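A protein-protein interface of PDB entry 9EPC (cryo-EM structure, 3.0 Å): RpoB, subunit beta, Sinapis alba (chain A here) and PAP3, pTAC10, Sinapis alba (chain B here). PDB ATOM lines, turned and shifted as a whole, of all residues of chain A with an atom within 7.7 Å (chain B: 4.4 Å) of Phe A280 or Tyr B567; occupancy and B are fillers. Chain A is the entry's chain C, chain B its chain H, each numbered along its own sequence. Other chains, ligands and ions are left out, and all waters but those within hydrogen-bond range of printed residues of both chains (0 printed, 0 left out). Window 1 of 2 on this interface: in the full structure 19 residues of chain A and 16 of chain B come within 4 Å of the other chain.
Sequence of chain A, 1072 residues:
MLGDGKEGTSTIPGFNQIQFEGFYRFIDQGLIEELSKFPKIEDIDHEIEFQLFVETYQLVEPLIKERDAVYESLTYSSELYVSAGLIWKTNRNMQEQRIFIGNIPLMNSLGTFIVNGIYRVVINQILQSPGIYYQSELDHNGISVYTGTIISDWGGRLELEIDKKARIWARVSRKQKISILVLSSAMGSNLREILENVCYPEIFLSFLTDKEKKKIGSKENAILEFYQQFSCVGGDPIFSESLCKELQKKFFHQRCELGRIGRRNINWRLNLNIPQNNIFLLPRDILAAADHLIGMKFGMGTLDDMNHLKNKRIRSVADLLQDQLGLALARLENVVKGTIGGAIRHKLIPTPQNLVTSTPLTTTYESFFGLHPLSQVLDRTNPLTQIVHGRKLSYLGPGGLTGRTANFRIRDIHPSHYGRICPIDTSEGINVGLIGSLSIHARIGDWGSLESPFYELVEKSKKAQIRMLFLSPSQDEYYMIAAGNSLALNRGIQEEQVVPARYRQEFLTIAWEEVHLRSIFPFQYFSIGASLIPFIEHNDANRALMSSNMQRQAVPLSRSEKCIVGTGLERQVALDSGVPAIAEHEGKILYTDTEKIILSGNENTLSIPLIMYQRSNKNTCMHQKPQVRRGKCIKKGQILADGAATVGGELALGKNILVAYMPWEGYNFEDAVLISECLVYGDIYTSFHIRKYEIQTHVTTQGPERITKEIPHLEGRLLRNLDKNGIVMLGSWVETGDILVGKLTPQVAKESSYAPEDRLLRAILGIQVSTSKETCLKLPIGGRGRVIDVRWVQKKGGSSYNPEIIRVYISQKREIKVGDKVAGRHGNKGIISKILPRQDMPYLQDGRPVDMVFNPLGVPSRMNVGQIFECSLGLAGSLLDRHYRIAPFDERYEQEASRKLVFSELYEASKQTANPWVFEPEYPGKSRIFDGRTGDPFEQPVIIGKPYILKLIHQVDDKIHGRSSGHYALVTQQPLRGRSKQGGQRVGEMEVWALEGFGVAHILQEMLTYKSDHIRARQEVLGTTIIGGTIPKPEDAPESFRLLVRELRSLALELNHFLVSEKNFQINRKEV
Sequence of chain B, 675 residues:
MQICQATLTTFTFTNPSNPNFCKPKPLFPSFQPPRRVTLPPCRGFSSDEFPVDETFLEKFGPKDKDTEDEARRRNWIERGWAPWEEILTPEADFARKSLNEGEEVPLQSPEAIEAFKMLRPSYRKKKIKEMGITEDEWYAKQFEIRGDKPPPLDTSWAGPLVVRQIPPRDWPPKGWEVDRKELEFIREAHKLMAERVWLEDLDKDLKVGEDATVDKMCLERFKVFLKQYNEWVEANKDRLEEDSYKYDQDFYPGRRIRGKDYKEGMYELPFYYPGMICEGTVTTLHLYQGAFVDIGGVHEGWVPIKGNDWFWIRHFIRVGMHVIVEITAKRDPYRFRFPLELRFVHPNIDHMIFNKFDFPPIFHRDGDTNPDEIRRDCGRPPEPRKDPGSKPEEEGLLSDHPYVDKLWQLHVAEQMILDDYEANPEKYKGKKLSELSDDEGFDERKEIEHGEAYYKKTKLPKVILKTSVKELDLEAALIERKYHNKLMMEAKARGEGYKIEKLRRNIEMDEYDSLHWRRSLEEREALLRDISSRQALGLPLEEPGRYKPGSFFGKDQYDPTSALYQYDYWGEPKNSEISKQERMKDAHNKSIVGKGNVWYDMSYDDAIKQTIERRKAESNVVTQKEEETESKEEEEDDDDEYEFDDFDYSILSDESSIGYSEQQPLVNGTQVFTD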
ATOM      1  N   MET A 187     -25.910  28.319  -0.987  1.00  0.00           N
ATOM      2  CA  MET A 187     -26.465  27.027  -0.601  1.00  0.00           C
ATOM      3  C   MET A 187     -25.890  26.548   0.730  1.00  0.00           C
ATOM      4  O   MET A 187     -26.590  26.530   1.749  1.00  0.00           O
ATOM      5  CB  MET A 187     -26.207  26.009  -1.713  1.00  0.00           C
ATOM      6  CG  MET A 187     -26.308  26.581  -3.127  1.00  0.00           C
ATOM      7  SD  MET A 187     -25.373  25.667  -4.364  1.00  0.00           S
ATOM      8  CE  MET A 187     -23.699  25.999  -3.816  1.00  0.00           C
ATOM      9  N   GLY A 188     -24.617  26.168   0.742  1.00  0.00           N
ATOM     10  CA  GLY A 188     -23.950  25.758   1.960  1.00  0.00           C
ATOM     11  C   GLY A 188     -22.508  26.218   2.003  1.00  0.00           C
ATOM     12  O   GLY A 188     -21.749  25.821   2.891  1.00  0.00           O
ATOM     13  N   PHE A 252     -32.897  22.602  -5.166  1.00  0.00           N
ATOM     14  CA  PHE A 252     -32.263  21.514  -4.430  1.00  0.00           C
ATOM     15  C   PHE A 252     -31.942  20.337  -5.344  1.00  0.00           C
ATOM     16  O   PHE A 252     -30.851  19.761  -5.263  1.00  0.00           O
ATOM     17  CB  PHE A 252     -33.154  21.076  -3.264  1.00  0.00           C
ATOM     18  CG  PHE A 252     -34.569  20.749  -3.660  1.00  0.00           C
ATOM     19  CD1 PHE A 252     -35.533  21.743  -3.729  1.00  0.00           C
ATOM     20  CD2 PHE A 252     -34.940  19.445  -3.947  1.00  0.00           C
ATOM     21  CE1 PHE A 252     -36.834  21.444  -4.089  1.00  0.00           C
ATOM     22  CE2 PHE A 252     -36.240  19.142  -4.309  1.00  0.00           C
ATOM     23  CZ  PHE A 252     -37.188  20.142  -4.378  1.00  0.00           C
ATOM     24  N   HIS A 253     -32.874  19.969  -6.221  1.00  0.00           N
ATOM     25  CA  HIS A 253     -32.689  18.829  -7.111  1.00  0.00           C
ATOM     26  C   HIS A 253     -33.084  19.094  -8.556  1.00  0.00           C
ATOM     27  O   HIS A 253     -32.666  18.324  -9.432  1.00  0.00           O
ATOM     28  CB  HIS A 253     -33.481  17.616  -6.597  1.00  0.00           C
ATOM     29  CG  HIS A 253     -33.198  16.347  -7.339  1.00  0.00           C
ATOM     30  ND1 HIS A 253     -32.080  16.178  -8.127  1.00  0.00           N
ATOM     31  CD2 HIS A 253     -33.892  15.187  -7.416  1.00  0.00           C
ATOM     32  CE1 HIS A 253     -32.096  14.967  -8.656  1.00  0.00           C
ATOM     33  NE2 HIS A 253     -33.185  14.346  -8.241  1.00  0.00           N
ATOM     34  N   CYS A 256     -29.446  21.042 -10.127  1.00  0.00           N
ATOM     35  CA  CYS A 256     -28.358  21.161  -9.162  1.00  0.00           C
ATOM     36  C   CYS A 256     -27.229  20.165  -9.376  1.00  0.00           C
ATOM     37  O   CYS A 256     -26.144  20.371  -8.825  1.00  0.00           O
ATOM     38  CB  CYS A 256     -28.894  21.005  -7.733  1.00  0.00           C
ATOM     39  SG  CYS A 256     -27.739  21.475  -6.421  1.00  0.00           S
ATOM     40  N   GLU A 257     -27.427  19.104 -10.153  1.00  0.00           N
ATOM     41  CA  GLU A 257     -26.392  18.117 -10.422  1.00  0.00           C
ATOM     42  C   GLU A 257     -26.067  18.117 -11.909  1.00  0.00           C
ATOM     43  O   GLU A 257     -26.955  18.292 -12.749  1.00  0.00           O
ATOM     44  CB  GLU A 257     -26.828  16.717  -9.969  1.00  0.00           C
ATOM     45  CG  GLU A 257     -27.868  16.033 -10.855  1.00  0.00           C
ATOM     46  CD  GLU A 257     -29.209  16.742 -10.859  1.00  0.00           C
ATOM     47  OE1 GLU A 257     -29.496  17.491  -9.901  1.00  0.00           O
ATOM     48  OE2 GLU A 257     -29.977  16.552 -11.827  1.00  0.00           O
ATOM     49  N   LEU A 258     -24.789  17.938 -12.229  1.00  0.00           N
ATOM     50  CA  LEU A 258     -24.347  17.957 -13.615  1.00  0.00           C
ATOM     51  C   LEU A 258     -24.376  16.586 -14.273  1.00  0.00           C
ATOM     52  O   LEU A 258     -24.292  16.506 -15.502  1.00  0.00           O
ATOM     53  CB  LEU A 258     -22.933  18.532 -13.709  1.00  0.00           C
ATOM     54  CG  LEU A 258     -22.776  19.961 -13.192  1.00  0.00           C
ATOM     55  CD1 LEU A 258     -21.364  20.456 -13.431  1.00  0.00           C
ATOM     56  CD2 LEU A 258     -23.789  20.882 -13.850  1.00  0.00           C
ATOM     57  N   GLY A 259     -24.494  15.515 -13.498  1.00  0.00           N
ATOM     58  CA  GLY A 259     -24.494  14.184 -14.063  1.00  0.00           C
ATOM     59  C   GLY A 259     -23.101  13.730 -14.446  1.00  0.00           C
ATOM     60  O   GLY A 259     -22.100  14.425 -14.263  1.00  0.00           O
ATOM     61  N   ARG A 263     -20.062  16.563 -15.349  1.00  0.00           N
ATOM     62  CA  ARG A 263     -18.838  16.633 -14.558  1.00  0.00           C
ATOM     63  C   ARG A 263     -17.605  16.587 -15.449  1.00  0.00           C
ATOM     64  O   ARG A 263     -16.619  17.289 -15.196  1.00  0.00           O
ATOM     65  CB  ARG A 263     -18.807  15.501 -13.533  1.00  0.00           C
ATOM     66  CG  ARG A 263     -17.549  15.469 -12.678  1.00  0.00           C
ATOM     67  CD  ARG A 263     -17.276  16.819 -12.037  1.00  0.00           C
ATOM     68  NE  ARG A 263     -18.379  17.260 -11.192  1.00  0.00           N
ATOM     69  CZ  ARG A 263     -18.460  18.461 -10.637  1.00  0.00           C
ATOM     70  NH1 ARG A 263     -17.521  19.374 -10.824  1.00  0.00           N
ATOM     71  NH2 ARG A 263     -19.512  18.754  -9.878  1.00  0.00           N
ATOM     72  N   ILE A 266     -17.511  20.107 -17.250  1.00  0.00           N
ATOM     73  CA  ILE A 266     -17.186  21.216 -16.362  1.00  0.00           C
ATOM     74  C   ILE A 266     -15.716  21.169 -15.962  1.00  0.00           C
ATOM     75  O   ILE A 266     -15.077  22.215 -15.799  1.00  0.00           O
ATOM     76  CB  ILE A 266     -18.120  21.223 -15.134  1.00  0.00           C
ATOM     77  CG1 ILE A 266     -18.012  22.550 -14.385  1.00  0.00           C
ATOM     78  CG2 ILE A 266     -17.812  20.077 -14.194  1.00  0.00           C
ATOM     79  CD1 ILE A 266     -18.696  23.693 -15.085  1.00  0.00           C
ATOM     80  N   ILE A 274     -11.709  18.076  -9.405  1.00  0.00           N
ATOM     81  CA  ILE A 274     -12.785  17.284  -8.797  1.00  0.00           C
ATOM     82  C   ILE A 274     -12.935  15.971  -9.557  1.00  0.00           C
ATOM     83  O   ILE A 274     -13.067  15.983 -10.796  1.00  0.00           O
ATOM     84  CB  ILE A 274     -14.102  18.080  -8.798  1.00  0.00           C
ATOM     85  CG1 ILE A 274     -15.304  17.150  -8.622  1.00  0.00           C
ATOM     86  CG2 ILE A 274     -14.228  18.907 -10.064  1.00  0.00           C
ATOM     87  CD1 ILE A 274     -15.486  16.650  -7.213  1.00  0.00           C
ATOM     88  N   PRO A 275     -12.899  14.820  -8.884  1.00  0.00           N
ATOM     89  CA  PRO A 275     -13.015  13.543  -9.596  1.00  0.00           C
ATOM     90  C   PRO A 275     -14.369  13.388 -10.271  1.00  0.00           C
ATOM     91  O   PRO A 275     -15.382  13.928  -9.821  1.00  0.00           O
ATOM     92  CB  PRO A 275     -12.824  12.499  -8.489  1.00  0.00           C
ATOM     93  CG  PRO A 275     -12.090  13.218  -7.410  1.00  0.00           C
ATOM     94  CD  PRO A 275     -12.583  14.631  -7.458  1.00  0.00           C
ATOM     95  N   GLN A 276     -14.372  12.630 -11.370  1.00  0.00           N
ATOM     96  CA  GLN A 276     -15.591  12.410 -12.138  1.00  0.00           C
ATOM     97  C   GLN A 276     -16.626  11.593 -11.374  1.00  0.00           C
ATOM     98  O   GLN A 276     -17.797  11.582 -11.768  1.00  0.00           O
ATOM     99  CB  GLN A 276     -15.263  11.714 -13.459  1.00  0.00           C
ATOM    100  CG  GLN A 276     -15.063  10.209 -13.343  1.00  0.00           C
ATOM    101  CD  GLN A 276     -13.882   9.832 -12.470  1.00  0.00           C
ATOM    102  OE1 GLN A 276     -12.939  10.608 -12.309  1.00  0.00           O
ATOM    103  NE2 GLN A 276     -13.932   8.637 -11.894  1.00  0.00           N
ATOM    104  N   ASN A 277     -16.221  10.903 -10.306  1.00  0.00           N
ATOM    105  CA  ASN A 277     -17.176  10.116  -9.533  1.00  0.00           C
ATOM    106  C   ASN A 277     -18.245  11.002  -8.914  1.00  0.00           C
ATOM    107  O   ASN A 277     -19.428  10.643  -8.897  1.00  0.00           O
ATOM    108  CB  ASN A 277     -16.447   9.318  -8.452  1.00  0.00           C
ATOM    109  CG  ASN A 277     -15.509   8.281  -9.031  1.00  0.00           C
ATOM    110  OD1 ASN A 277     -15.783   7.696 -10.078  1.00  0.00           O
ATOM    111  ND2 ASN A 277     -14.393   8.047  -8.351  1.00  0.00           N
ATOM    112  N   ASN A 278     -17.851  12.161  -8.397  1.00  0.00           N
ATOM    113  CA  ASN A 278     -18.822  13.092  -7.848  1.00  0.00           C
ATOM    114  C   ASN A 278     -19.703  13.645  -8.961  1.00  0.00           C
ATOM    115  O   ASN A 278     -19.229  13.967 -10.053  1.00  0.00           O
ATOM    116  CB  ASN A 278     -18.119  14.230  -7.112  1.00  0.00           C
ATOM    117  CG  ASN A 278     -19.055  15.006  -6.204  1.00  0.00           C
ATOM    118  OD1 ASN A 278     -20.199  15.289  -6.561  1.00  0.00           O
ATOM    119  ND2 ASN A 278     -18.571  15.348  -5.015  1.00  0.00           N
ATOM    120  N   ILE A 279     -20.996  13.753  -8.671  1.00  0.00           N
ATOM    121  CA  ILE A 279     -21.984  14.205  -9.634  1.00  0.00           C
ATOM    122  C   ILE A 279     -22.531  15.579  -9.271  1.00  0.00           C
ATOM    123  O   ILE A 279     -22.764  16.412 -10.151  1.00  0.00           O
ATOM    124  CB  ILE A 279     -23.125  13.169  -9.746  1.00  0.00           C
ATOM    125  CG1 ILE A 279     -22.594  11.848 -10.305  1.00  0.00           C
ATOM    126  CG2 ILE A 279     -24.274  13.705 -10.578  1.00  0.00           C
ATOM    127  CD1 ILE A 279     -21.876  11.985 -11.631  1.00  0.00           C
ATOM    128  N   PHE A 280     -22.733  15.829  -7.982  1.00  0.00           N
ATOM    129  CA  PHE A 280     -23.342  17.070  -7.528  1.00  0.00           C
ATOM    130  C   PHE A 280     -22.433  18.261  -7.806  1.00  0.00           C
ATOM    131  O   PHE A 280     -21.206  18.168  -7.713  1.00  0.00           O
ATOM    132  CB  PHE A 280     -23.655  16.971  -6.036  1.00  0.00           C
ATOM    133  CG  PHE A 280     -24.004  15.582  -5.593  1.00  0.00           C
ATOM    134  CD1 PHE A 280     -25.296  15.109  -5.711  1.00  0.00           C
ATOM    135  CD2 PHE A 280     -23.024  14.738  -5.079  1.00  0.00           C
ATOM    136  CE1 PHE A 280     -25.614  13.831  -5.318  1.00  0.00           C
ATOM    137  CE2 PHE A 280     -23.333  13.458  -4.683  1.00  0.00           C
ATOM    138  CZ  PHE A 280     -24.643  13.007  -4.800  1.00  0.00           C
ATOM    139  N   LEU A 281     -23.051  19.386  -8.150  1.00  0.00           N
ATOM    140  CA  LEU A 281     -22.307  20.610  -8.402  1.00  0.00           C
ATOM    141  C   LEU A 281     -21.632  21.099  -7.123  1.00  0.00           C
ATOM    142  O   LEU A 281     -22.101  20.850  -6.010  1.00  0.00           O
ATOM    143  CB  LEU A 281     -23.240  21.689  -8.953  1.00  0.00           C
ATOM    144  CG  LEU A 281     -22.640  23.010  -9.439  1.00  0.00           C
ATOM    145  CD1 LEU A 281     -21.689  22.769 -10.595  1.00  0.00           C
ATOM    146  CD2 LEU A 281     -23.740  23.978  -9.845  1.00  0.00           C
ATOM    147  N   LEU A 282     -20.512  21.797  -7.293  1.00  0.00           N
ATOM    148  CA  LEU A 282     -19.765  22.310  -6.158  1.00  0.00           C
ATOM    149  C   LEU A 282     -19.601  23.821  -6.264  1.00  0.00           C
ATOM    150  O   LEU A 282     -19.539  24.366  -7.371  1.00  0.00           O
ATOM    151  CB  LEU A 282     -18.381  21.655  -6.061  1.00  0.00           C
ATOM    152  CG  LEU A 282     -18.366  20.144  -5.828  1.00  0.00           C
ATOM    153  CD1 LEU A 282     -16.940  19.649  -5.649  1.00  0.00           C
ATOM    154  CD2 LEU A 282     -19.219  19.783  -4.623  1.00  0.00           C
ATOM    155  N   PRO A 283     -19.534  24.527  -5.131  1.00  0.00           N
ATOM    156  CA  PRO A 283     -19.267  25.973  -5.195  1.00  0.00           C
ATOM    157  C   PRO A 283     -17.922  26.294  -5.815  1.00  0.00           C
ATOM    158  O   PRO A 283     -17.732  27.403  -6.329  1.00  0.00           O
ATOM    159  CB  PRO A 283     -19.340  26.410  -3.725  1.00  0.00           C
ATOM    160  CG  PRO A 283     -19.071  25.170  -2.947  1.00  0.00           C
ATOM    161  CD  PRO A 283     -19.667  24.050  -3.745  1.00  0.00           C
ATOM    162  N   ASP A 285     -16.914  24.867  -8.543  1.00  0.00           N
ATOM    163  CA  ASP A 285     -17.269  24.990  -9.952  1.00  0.00           C
ATOM    164  C   ASP A 285     -17.876  26.354 -10.247  1.00  0.00           C
ATOM    165  O   ASP A 285     -17.556  26.979 -11.265  1.00  0.00           O
ATOM    166  CB  ASP A 285     -18.237  23.875 -10.344  1.00  0.00           C
ATOM    167  CG  ASP A 285     -17.869  22.540  -9.725  1.00  0.00           C
ATOM    168  OD1 ASP A 285     -16.672  22.323  -9.446  1.00  0.00           O
ATOM    169  OD2 ASP A 285     -18.778  21.712  -9.512  1.00  0.00           O
ATOM    170  N   TYR B 565     -15.461  22.076  -1.522  1.00  0.00           N
ATOM    171  CA  TYR B 565     -15.819  20.840  -2.200  1.00  0.00           C
ATOM    172  C   TYR B 565     -16.995  20.123  -1.551  1.00  0.00           C
ATOM    173  O   TYR B 565     -17.360  19.032  -2.000  1.00  0.00           O
ATOM    174  CB  TYR B 565     -14.609  19.900  -2.252  1.00  0.00           C
ATOM    175  CG  TYR B 565     -13.401  20.491  -2.944  1.00  0.00           C
ATOM    176  CD1 TYR B 565     -12.476  21.249  -2.240  1.00  0.00           C
ATOM    177  CD2 TYR B 565     -13.184  20.286  -4.299  1.00  0.00           C
ATOM    178  CE1 TYR B 565     -11.370  21.791  -2.867  1.00  0.00           C
ATOM    179  CE2 TYR B 565     -12.080  20.821  -4.935  1.00  0.00           C
ATOM    180  CZ  TYR B 565     -11.177  21.573  -4.215  1.00  0.00           C
ATOM    181  OH  TYR B 565     -10.077  22.108  -4.843  1.00  0.00           O
ATOM    182  N   GLN B 566     -17.592  20.699  -0.511  1.00  0.00           N
ATOM    183  CA  GLN B 566     -18.715  20.070   0.169  1.00  0.00           C
ATOM    184  C   GLN B 566     -19.984  20.204  -0.662  1.00  0.00           C
ATOM    185  O   GLN B 566     -20.243  21.258  -1.251  1.00  0.00           O
ATOM    186  CB  GLN B 566     -18.921  20.694   1.549  1.00  0.00           C
ATOM    187  CG  GLN B 566     -18.083  20.064   2.642  1.00  0.00           C
ATOM    188  CD  GLN B 566     -18.479  18.628   2.923  1.00  0.00           C
ATOM    189  OE1 GLN B 566     -19.627  18.233   2.711  1.00  0.00           O
ATOM    190  NE2 GLN B 566     -17.528  17.836   3.403  1.00  0.00           N
ATOM    191  N   TYR B 567     -20.776  19.130  -0.706  1.00  0.00           N
ATOM    192  CA  TYR B 567     -22.036  19.108  -1.439  1.00  0.00           C
ATOM    193  C   TYR B 567     -23.235  18.911  -0.514  1.00  0.00           C
ATOM    194  O   TYR B 567     -24.268  18.382  -0.929  1.00  0.00           O
ATOM    195  CB  TYR B 567     -22.011  18.020  -2.513  1.00  0.00           C
ATOM    196  CG  TYR B 567     -21.781  16.616  -1.985  1.00  0.00           C
ATOM    197  CD1 TYR B 567     -20.491  16.110  -1.838  1.00  0.00           C
ATOM    198  CD2 TYR B 567     -22.851  15.795  -1.643  1.00  0.00           C
ATOM    199  CE1 TYR B 567     -20.275  14.832  -1.358  1.00  0.00           C
ATOM    200  CE2 TYR B 567     -22.644  14.518  -1.162  1.00  0.00           C
ATOM    201  CZ  TYR B 567     -21.357  14.038  -1.030  1.00  0.00           C
ATOM    202  OH  TYR B 567     -21.152  12.765  -0.551  1.00  0.00           O
ATOM    203  N   ASP B 568     -23.127  19.377   0.729  1.00  0.00           N
ATOM    204  CA  ASP B 568     -24.156  19.185   1.748  1.00  0.00           C
ATOM    205  C   ASP B 568     -25.015  20.428   1.922  1.00  0.00           C
ATOM    206  O   ASP B 568     -25.325  20.830   3.047  1.00  0.00           O
ATOM    207  CB  ASP B 568     -23.523  18.774   3.075  1.00  0.00           C
ATOM    208  CG  ASP B 568     -22.428  19.722   3.520  1.00  0.00           C
ATOM    209  OD1 ASP B 568     -22.074  20.633   2.742  1.00  0.00           O
ATOM    210  OD2 ASP B 568     -21.919  19.553   4.650  1.00  0.00           O
ATOM    211  N   TYR B 569     -25.385  21.057   0.803  1.00  0.00           N
ATOM    212  CA  TYR B 569     -26.092  22.335   0.822  1.00  0.00           C
ATOM    213  C   TYR B 569     -27.316  22.291   1.730  1.00  0.00           C
ATOM    214  O   TYR B 569     -27.394  23.012   2.731  1.00  0.00           O
ATOM    215  CB  TYR B 569     -26.510  22.710  -0.601  1.00  0.00           C
ATOM    216  CG  TYR B 569     -25.405  22.659  -1.633  1.00  0.00           C
ATOM    217  CD1 TYR B 569     -24.067  22.758  -1.268  1.00  0.00           C
ATOM    218  CD2 TYR B 569     -25.705  22.521  -2.981  1.00  0.00           C
ATOM    219  CE1 TYR B 569     -23.064  22.710  -2.214  1.00  0.00           C
ATOM    220  CE2 TYR B 569     -24.711  22.476  -3.933  1.00  0.00           C
ATOM    221  CZ  TYR B 569     -23.394  22.570  -3.544  1.00  0.00           C
ATOM    222  OH  TYR B 569     -22.407  22.526  -4.497  1.00  0.00           O
ATOM    223  N   PRO B 573     -28.170  14.757  -0.394  1.00  0.00           N
ATOM    224  CA  PRO B 573     -29.177  14.351  -1.380  1.00  0.00           C
ATOM    225  C   PRO B 573     -29.341  12.840  -1.423  1.00  0.00           C
ATOM    226  O   PRO B 573     -28.402  12.081  -1.169  1.00  0.00           O
ATOM    227  CB  PRO B 573     -28.625  14.898  -2.702  1.00  0.00           C
ATOM    228  CG  PRO B 573     -27.167  15.104  -2.456  1.00  0.00           C
ATOM    229  CD  PRO B 573     -27.038  15.466  -1.011  1.00  0.00           C
ATOM    230  N   ASN B 575     -29.517  10.889  -3.800  1.00  0.00           N
ATOM    231  CA  ASN B 575     -28.692  10.246  -4.812  1.00  0.00           C
ATOM    232  C   ASN B 575     -27.225  10.175  -4.413  1.00  0.00           C
ATOM    233  O   ASN B 575     -26.398   9.747  -5.224  1.00  0.00           O
ATOM    234  CB  ASN B 575     -28.834  10.972  -6.151  1.00  0.00           C
ATOM    235  CG  ASN B 575     -30.190  10.750  -6.790  1.00  0.00           C
ATOM    236  OD1 ASN B 575     -31.164  10.431  -6.109  1.00  0.00           O
ATOM    237  ND2 ASN B 575     -30.258  10.912  -8.105  1.00  0.00           N
ATOM    238  N   SER B 576     -26.884  10.597  -3.198  1.00  0.00           N
ATOM    239  CA  SER B 576     -25.510  10.486  -2.729  1.00  0.00           C
ATOM    240  C   SER B 576     -25.089   9.027  -2.694  1.00  0.00           C
ATOM    241  O   SER B 576     -25.795   8.181  -2.137  1.00  0.00           O
ATOM    242  CB  SER B 576     -25.367  11.116  -1.345  1.00  0.00           C
ATOM    243  OG  SER B 576     -25.610  12.509  -1.387  1.00  0.00           O
ATOM    244  N   GLU B 577     -23.936   8.732  -3.296  1.00  0.00           N
ATOM    245  CA  GLU B 577     -23.426   7.368  -3.244  1.00  0.00           C
ATOM    246  C   GLU B 577     -23.077   6.971  -1.818  1.00  0.00           C
ATOM    247  O   GLU B 577     -23.171   5.792  -1.463  1.00  0.00           O
ATOM    248  CB  GLU B 577     -22.215   7.213  -4.168  1.00  0.00           C
ATOM    249  CG  GLU B 577     -20.908   7.781  -3.628  1.00  0.00           C
ATOM    250  CD  GLU B 577     -20.901   9.295  -3.557  1.00  0.00           C
ATOM    251  OE1 GLU B 577     -21.779   9.930  -4.178  1.00  0.00           O
ATOM    252  OE2 GLU B 577     -20.014   9.852  -2.878  1.00  0.00           O
ATOM    253  N   ILE B 578     -22.680   7.937  -0.986  1.00  0.00           N
ATOM    254  CA  ILE B 578     -22.450   7.641   0.422  1.00  0.00           C
ATOM    255  C   ILE B 578     -23.773   7.388   1.136  1.00  0.00           C
ATOM    256  O   ILE B 578     -23.883   6.469   1.955  1.00  0.00           O
ATOM    257  CB  ILE B 578     -21.640   8.770   1.086  1.00  0.00           C
ATOM    258  CG1 ILE B 578     -22.329  10.126   0.909  1.00  0.00           C
ATOM    259  CG2 ILE B 578     -20.232   8.815   0.517  1.00  0.00           C
ATOM    260  CD1 ILE B 578     -23.050  10.613   2.149  1.00  0.00           C
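N of Leu A281 lies close to O of Cys A256, 3.3 Å away. The guanidinium group (NH2) of Arg A263 lies within hydrogen-bond range of the backbone carbonyl oxygen (O) of Phe A280 (2.8 Å). The side-chain amide oxygen (OD1) of Asn A278 is in hydrogen-bond range of the backbone NH (N) of Phe A280 (3.0 Å). N of Leu A282 sits at hydrogen-bond distance from OD2 of Asp A285 (2.8 Å). OE1 of Gln B566 lies close to OD2 of Asp B568 (3.3 Å). The backbone carbonyl oxygen (O) of Pro B573 lies within hydrogen-bond range of the side-chain hydroxyl (OG) of Ser B576 (2.8 Å).
Of the 21 printed residues of chain A, 7 touch a printed residue of chain B. Among the printed residues, 15 pairs touch across the chains. Among the printed residues, no Asp or Glu carboxylate lies within 4 Å of a Lys or Arg side-chain nitrogen of the other chain.
The side-chain hydroxyl (OH) of Tyr B569 lies close to the backbone NH (N) of Leu A282 (3.5 Å). The backbone carbonyl oxygen (O) of Leu A281 lies close to the side-chain hydroxyl (OH) of Tyr B569, 2.3 Å away.
Phe A280 touches just these residues of chain B: Tyr B567 (3.6 Å), Pro B573 (3.5 Å), Asn B575 (3.7 Å), Ser B576 (3.4 Å) and Glu B577 (3.9 Å). Of the printed residues of chain A, Tyr B567 touches Asn A278, Phe A280 and Leu A282. Of the printed residues of chain A, Ser B576 touches Phe A280 (3.4 Å). Of the printed residues of chain B, Asn A278 touches Tyr B567. Of the printed residues of chain B, Met A187 touches Tyr B569. Of the printed residues of chain A, Tyr B569 touches Met A187 (3.3 Å), Gly A188 (3.996 Å), Leu A281 (2.3 Å), Leu A282 (3.1 Å) and Pro A283 (3.2 Å). Printed residues of chain A within 4 Å of Tyr B565: Leu A282 (3.3 Å). Ile A274 touches none of the printed residues of chain B. The nearest residue of chain A that does not touch Tyr B567 is Leu A281 (4.5 Å).
Met A187 touches Tyr B569. Tyr B569 touches Gly A188. CD2 of Phe A280 touches CD2 of Tyr B567, at 3.6 Å. Phe A280 touches Pro B573 (CE1 to CG, 3.5 Å). CZ of Phe A280 touches O of Asn B575 (3.7 Å). Phe A280 touches Ser B576. Glu B577 touches Phe A280. Leu A282 touches Tyr B565 (CD2 to O, 3.3 Å). CB of Tyr B567 touches CD2 of Leu A282 (3.9 Å). Tyr B569 touches Pro A283.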
